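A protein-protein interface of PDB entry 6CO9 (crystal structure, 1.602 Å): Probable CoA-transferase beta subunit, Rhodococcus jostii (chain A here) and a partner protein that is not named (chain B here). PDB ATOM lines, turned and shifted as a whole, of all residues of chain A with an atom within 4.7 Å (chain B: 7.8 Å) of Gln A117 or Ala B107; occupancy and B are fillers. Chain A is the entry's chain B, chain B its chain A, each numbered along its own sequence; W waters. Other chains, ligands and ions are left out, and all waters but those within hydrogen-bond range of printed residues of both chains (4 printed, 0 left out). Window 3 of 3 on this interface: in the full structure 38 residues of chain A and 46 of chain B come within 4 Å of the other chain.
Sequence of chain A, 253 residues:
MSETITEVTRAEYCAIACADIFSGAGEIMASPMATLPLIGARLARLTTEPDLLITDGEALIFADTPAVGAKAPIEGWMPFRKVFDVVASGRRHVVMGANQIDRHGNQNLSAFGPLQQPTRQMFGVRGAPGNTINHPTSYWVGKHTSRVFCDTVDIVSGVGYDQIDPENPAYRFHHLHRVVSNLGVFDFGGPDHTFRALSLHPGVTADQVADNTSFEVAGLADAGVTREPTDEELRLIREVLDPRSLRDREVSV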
ATOM      1  N   PRO A 114     -13.158  11.330 -21.955  1.00  0.00           N
ATOM      2  CA  PRO A 114     -12.471  10.668 -20.838  1.00  0.00           C
ATOM      3  C   PRO A 114     -12.203  11.620 -19.681  1.00  0.00           C
ATOM      4  O   PRO A 114     -11.929  12.807 -19.877  1.00  0.00           O
ATOM      5  CB  PRO A 114     -11.158  10.184 -21.465  1.00  0.00           C
ATOM      6  CG  PRO A 114     -11.444  10.107 -22.928  1.00  0.00           C
ATOM      7  CD  PRO A 114     -12.392  11.229 -23.206  1.00  0.00           C
ATOM      8  N   LEU A 115     -12.257  11.063 -18.462  1.00  0.00           N
ATOM      9  CA  LEU A 115     -12.154  11.867 -17.244  1.00  0.00           C
ATOM     10  C   LEU A 115     -10.877  12.696 -17.199  1.00  0.00           C
ATOM     11  O   LEU A 115     -10.901  13.853 -16.761  1.00  0.00           O
ATOM     12  CB  LEU A 115     -12.196  10.971 -16.005  1.00  0.00           C
ATOM     13  CG  LEU A 115     -13.462  10.211 -15.642  1.00  0.00           C
ATOM     14  CD1 LEU A 115     -13.514  10.008 -14.138  1.00  0.00           C
ATOM     15  CD2 LEU A 115     -14.668  10.952 -16.108  1.00  0.00           C
ATOM     16  N   GLN A 116      -9.740  12.100 -17.557  1.00  0.00           N
ATOM     17  CA  GLN A 116      -8.460  12.785 -17.420  1.00  0.00           C
ATOM     18  C   GLN A 116      -8.010  13.477 -18.700  1.00  0.00           C
ATOM     19  O   GLN A 116      -6.984  14.162 -18.684  1.00  0.00           O
ATOM     20  CB  GLN A 116      -7.371  11.813 -16.945  1.00  0.00           C
ATOM     21  CG  GLN A 116      -7.625  11.256 -15.545  1.00  0.00           C
ATOM     22  CD  GLN A 116      -7.549  12.321 -14.459  1.00  0.00           C
ATOM     23  OE1 GLN A 116      -6.860  13.326 -14.606  1.00  0.00           O
ATOM     24  NE2 GLN A 116      -8.278  12.105 -13.357  1.00  0.00           N
ATOM     25  N   GLN A 117      -8.740  13.312 -19.799  1.00  0.00           N
ATOM     26  CA  GLN A 117      -8.469  14.060 -21.029  1.00  0.00           C
ATOM     27  C   GLN A 117      -9.770  14.200 -21.800  1.00  0.00           C
ATOM     28  O   GLN A 117     -10.018  13.495 -22.790  1.00  0.00           O
ATOM     29  CB  GLN A 117      -7.390  13.382 -21.872  1.00  0.00           C
ATOM     30  CG  GLN A 117      -7.039  14.196 -23.098  1.00  0.00           C
ATOM     31  CD  GLN A 117      -5.727  13.781 -23.740  1.00  0.00           C
ATOM     32  OE1 GLN A 117      -5.130  12.779 -23.365  1.00  0.00           O
ATOM     33  NE2 GLN A 117      -5.281  14.550 -24.723  1.00  0.00           N
ATOM     34  N   PRO A 118     -10.651  15.097 -21.356  1.00  0.00           N
ATOM     35  CA  PRO A 118     -11.953  15.254 -22.012  1.00  0.00           C
ATOM     36  C   PRO A 118     -11.821  15.808 -23.424  1.00  0.00           C
ATOM     37  O   PRO A 118     -10.810  16.405 -23.805  1.00  0.00           O
ATOM     38  CB  PRO A 118     -12.687  16.242 -21.096  1.00  0.00           C
ATOM     39  CG  PRO A 118     -11.597  17.001 -20.411  1.00  0.00           C
ATOM     40  CD  PRO A 118     -10.527  15.974 -20.174  1.00  0.00           C
ATOM     41  N   THR A 119     -12.872  15.589 -24.215  1.00  0.00           N
ATOM     42  CA  THR A 119     -12.952  16.209 -25.529  1.00  0.00           C
ATOM     43  C   THR A 119     -13.571  17.597 -25.473  1.00  0.00           C
ATOM     44  O   THR A 119     -13.370  18.393 -26.394  1.00  0.00           O
ATOM     45  CB  THR A 119     -13.744  15.320 -26.491  1.00  0.00           C
ATOM     46  OG1 THR A 119     -15.036  15.038 -25.938  1.00  0.00           O
ATOM     47  CG2 THR A 119     -12.999  14.006 -26.708  1.00  0.00           C
ATOM     48  N   PHE B 101      -7.907  26.615 -18.660  1.00  0.00           N
ATOM     49  CA  PHE B 101      -8.151  25.346 -17.990  1.00  0.00           C
ATOM     50  C   PHE B 101      -8.680  24.311 -18.980  1.00  0.00           C
ATOM     51  O   PHE B 101      -8.237  23.154 -18.978  1.00  0.00           O
ATOM     52  CB  PHE B 101      -9.111  25.576 -16.820  1.00  0.00           C
ATOM     53  CG  PHE B 101      -9.591  24.311 -16.148  1.00  0.00           C
ATOM     54  CD1 PHE B 101      -8.712  23.552 -15.400  1.00  0.00           C
ATOM     55  CD2 PHE B 101     -10.891  23.866 -16.317  1.00  0.00           C
ATOM     56  CE1 PHE B 101      -9.143  22.376 -14.778  1.00  0.00           C
ATOM     57  CE2 PHE B 101     -11.338  22.705 -15.681  1.00  0.00           C
ATOM     58  CZ  PHE B 101     -10.450  21.952 -14.934  1.00  0.00           C
ATOM     59  N   ALA B 102      -9.607  24.718 -19.851  1.00  0.00           N
ATOM     60  CA  ALA B 102     -10.160  23.791 -20.833  1.00  0.00           C
ATOM     61  C   ALA B 102      -9.076  23.244 -21.752  1.00  0.00           C
ATOM     62  O   ALA B 102      -9.070  22.048 -22.063  1.00  0.00           O
ATOM     63  CB  ALA B 102     -11.257  24.477 -21.653  1.00  0.00           C
ATOM     64  N   LYS B 103      -8.143  24.099 -22.187  1.00  0.00           N
ATOM     65  CA  LYS B 103      -7.058  23.636 -23.056  1.00  0.00           C
ATOM     66  C   LYS B 103      -6.162  22.637 -22.342  1.00  0.00           C
ATOM     67  O   LYS B 103      -5.737  21.636 -22.930  1.00  0.00           O
ATOM     68  CB  LYS B 103      -6.214  24.809 -23.555  1.00  0.00           C
ATOM     69  CG  LYS B 103      -6.921  25.814 -24.407  1.00  0.00           C
ATOM     70  CD  LYS B 103      -5.942  26.876 -24.861  1.00  0.00           C
ATOM     71  CE  LYS B 103      -6.640  27.888 -25.726  1.00  0.00           C
ATOM     72  NZ  LYS B 103      -6.640  27.497 -27.166  1.00  0.00           N
ATOM     73  N   ALA B 104      -5.808  22.922 -21.089  1.00  0.00           N
ATOM     74  CA  ALA B 104      -4.988  21.977 -20.341  1.00  0.00           C
ATOM     75  C   ALA B 104      -5.700  20.640 -20.198  1.00  0.00           C
ATOM     76  O   ALA B 104      -5.080  19.579 -20.336  1.00  0.00           O
ATOM     77  CB  ALA B 104      -4.631  22.551 -18.968  1.00  0.00           C
ATOM     78  N   ARG B 105      -7.014  20.677 -19.949  1.00  0.00           N
ATOM     79  CA  ARG B 105      -7.792  19.449 -19.800  1.00  0.00           C
ATOM     80  C   ARG B 105      -7.856  18.658 -21.101  1.00  0.00           C
ATOM     81  O   ARG B 105      -7.594  17.448 -21.118  1.00  0.00           O
ATOM     82  CB  ARG B 105      -9.197  19.795 -19.317  1.00  0.00           C
ATOM     83  CG  ARG B 105      -9.230  20.318 -17.896  1.00  0.00           C
ATOM     84  CD  ARG B 105      -9.175  19.161 -16.922  1.00  0.00           C
ATOM     85  NE  ARG B 105     -10.453  18.461 -16.886  1.00  0.00           N
ATOM     86  CZ  ARG B 105     -10.597  17.140 -16.807  1.00  0.00           C
ATOM     87  NH1 ARG B 105      -9.531  16.346 -16.775  1.00  0.00           N
ATOM     88  NH2 ARG B 105     -11.816  16.616 -16.774  1.00  0.00           N
ATOM     89  N   THR B 106      -8.231  19.314 -22.199  1.00  0.00           N
ATOM     90  CA  THR B 106      -8.372  18.591 -23.457  1.00  0.00           C
ATOM     91  C   THR B 106      -7.028  18.101 -23.981  1.00  0.00           C
ATOM     92  O   THR B 106      -6.992  17.135 -24.751  1.00  0.00           O
ATOM     93  CB  THR B 106      -9.087  19.463 -24.499  1.00  0.00           C
ATOM     94  OG1 THR B 106      -8.355  20.673 -24.719  1.00  0.00           O
ATOM     95  CG2 THR B 106     -10.501  19.807 -24.024  1.00  0.00           C
ATOM     96  N   ALA B 107      -5.927  18.709 -23.549  1.00  0.00           N
ATOM     97  CA  ALA B 107      -4.592  18.243 -23.900  1.00  0.00           C
ATOM     98  C   ALA B 107      -4.044  17.213 -22.920  1.00  0.00           C
ATOM     99  O   ALA B 107      -2.951  16.682 -23.147  1.00  0.00           O
ATOM    100  CB  ALA B 107      -3.628  19.431 -23.984  1.00  0.00           C
ATOM    101  N   GLY B 108      -4.772  16.914 -21.847  1.00  0.00           N
ATOM    102  CA  GLY B 108      -4.283  15.976 -20.853  1.00  0.00           C
ATOM    103  C   GLY B 108      -3.023  16.429 -20.152  1.00  0.00           C
ATOM    104  O   GLY B 108      -2.200  15.593 -19.763  1.00  0.00           O
ATOM    105  N   GLU B 109      -2.850  17.737 -19.975  1.00  0.00           N
ATOM    106  CA  GLU B 109      -1.646  18.276 -19.357  1.00  0.00           C
ATOM    107  C   GLU B 109      -1.692  18.265 -17.836  1.00  0.00           C
ATOM    108  O   GLU B 109      -0.649  18.450 -17.202  1.00  0.00           O
ATOM    109  CB  GLU B 109      -1.409  19.701 -19.850  1.00  0.00           C
ATOM    110  CG  GLU B 109      -1.053  19.741 -21.334  1.00  0.00           C
ATOM    111  CD  GLU B 109      -1.022  21.141 -21.912  1.00  0.00           C
ATOM    112  OE1 GLU B 109      -1.502  22.083 -21.252  1.00  0.00           O
ATOM    113  OE2 GLU B 109      -0.516  21.294 -23.045  1.00  0.00           O
ATOM    114  N   ILE B 110      -2.854  18.065 -17.231  1.00  0.00           N
ATOM    115  CA  ILE B 110      -2.966  18.080 -15.781  1.00  0.00           C
ATOM    116  C   ILE B 110      -3.706  16.830 -15.328  1.00  0.00           C
ATOM    117  O   ILE B 110      -4.608  16.339 -16.017  1.00  0.00           O
ATOM    118  CB  ILE B 110      -3.672  19.357 -15.279  1.00  0.00           C
ATOM    119  CG1 ILE B 110      -5.094  19.457 -15.820  1.00  0.00           C
ATOM    120  CG2 ILE B 110      -2.872  20.599 -15.670  1.00  0.00           C
ATOM    121  CD1 ILE B 110      -5.827  20.731 -15.326  1.00  0.00           C
ATOM    122  N   VAL B 112      -6.283  15.431 -12.674  1.00  0.00           N
ATOM    123  CA  VAL B 112      -7.311  16.105 -11.888  1.00  0.00           C
ATOM    124  C   VAL B 112      -7.845  15.186 -10.805  1.00  0.00           C
ATOM    125  O   VAL B 112      -8.052  13.982 -11.021  1.00  0.00           O
ATOM    126  CB  VAL B 112      -8.473  16.647 -12.745  1.00  0.00           C
ATOM    127  CG1 VAL B 112      -7.944  17.643 -13.771  1.00  0.00           C
ATOM    128  CG2 VAL B 112      -9.239  15.513 -13.415  1.00  0.00           C
ATOM    129  N   PHE B 147     -12.631   9.766 -10.673  1.00  0.00           N
ATOM    130  CA  PHE B 147     -11.564  10.762 -10.755  1.00  0.00           C
ATOM    131  C   PHE B 147     -10.423  10.429  -9.798  1.00  0.00           C
ATOM    132  O   PHE B 147      -9.245  10.635 -10.123  1.00  0.00           O
ATOM    133  CB  PHE B 147     -12.104  12.156 -10.423  1.00  0.00           C
ATOM    134  CG  PHE B 147     -12.780  12.861 -11.563  1.00  0.00           C
ATOM    135  CD1 PHE B 147     -12.059  13.295 -12.661  1.00  0.00           C
ATOM    136  CD2 PHE B 147     -14.136  13.141 -11.505  1.00  0.00           C
ATOM    137  CE1 PHE B 147     -12.687  13.976 -13.688  1.00  0.00           C
ATOM    138  CE2 PHE B 147     -14.771  13.814 -12.520  1.00  0.00           C
ATOM    139  CZ  PHE B 147     -14.042  14.238 -13.623  1.00  0.00           C
HETATM  140  O   HOH W   1      -9.457   9.393 -13.306  1.00  0.00           O
HETATM  141  O   HOH W   2      -4.315  13.828 -17.253  1.00  0.00           O
HETATM  142  O   HOH W   3      -6.740  16.776 -17.600  1.00  0.00           O
HETATM  143  O   HOH W   4      -9.039  15.835 -25.942  1.00  0.00           O
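O of Leu A115 touches CE1 of Phe B147 (3.6 Å). Arg B105 touches Gln A116 (NH1 to CA, 3.8 Å). CA of Gly B108 touches O of Gln A116, at 3.9 Å. Gln A116 touches Phe B147 (NE2 to O, 3.7 Å). Gln A117 touches Arg B105. Gln A117 touches Ala B107. Gln A117 touches Gly B108 (CG to N, 3.8 Å). Arg B105 touches Pro A118. Pro A118 touches Thr B106. Thr B106 touches Thr A119.
OG1 of Thr B106 sits at hydrogen-bond distance from O of Ala B102. OG1 of Thr B106 is in hydrogen-bond range of O of Lys B103, at 3.3 Å.
Gln A117 touches just these residues of chain B: Arg B105 (3.5 Å), Thr B106 (3.1 Å), Ala B107 (3.4 Å) and Gly B108 (3.8 Å). Of the printed residues of chain B, Thr A119 touches Thr B106. Of chain A, only Gln A117 comes within 4 Å of Ala B107. Printed residues of chain A within 4 Å of Gly B108: Gln A116 and Gln A117. Printed residues of chain A within 4 Å of Val B112: Gln A116 (2.9 Å).
Of the 12 printed residues of chain B, 6 touch a printed residue of chain A. Printed residues of chain B that touch a printed residue of chain A: Arg B105, Thr B106, Ala B107, Gly B108, Val B112 and Phe B147. Hydrophobic or aromatic side chains of chain B within 4 Å of the printed part of chain A: Val B112 and Phe B147. Of the 6 printed residues of chain A, 5 touch a printed residue of chain B. Printed residues of chain A that touch a printed residue of chain B: Leu A115, Gln A116, Gln A117, Pro A118 and Thr A119. Hydrophobic or aromatic side chains of chain A that line the printed part of chain B: Leu A115 and Pro A118.
Water W3 lies within hydrogen-bond range of O of Ile B110 (2.7 Å), O of Gln A116 (2.8 Å) and NH1 of Arg B105 (2.9 Å). Water W4 bridges O of Thr B106 (2.7 Å) and O of Pro A118 (2.8 Å). Water W2 bridges O of Ile B110 (2.8 Å) and O of Gln A116 (3.0 Å). Water W1 bridges NE2 of Gln A116 and O of Phe B147.
The guanidinium group of Arg B105 lies within hydrogen-bond range of the backbone carbonyl oxygen of Leu A115 (2.8 Å). O of Thr B106 lies within hydrogen-bond range of NE2 of Gln A117, at 3.1 Å. The side-chain amide oxygen (OE1) of Gln A116 is in hydrogen-bond range of the backbone NH (N) of Val B112.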
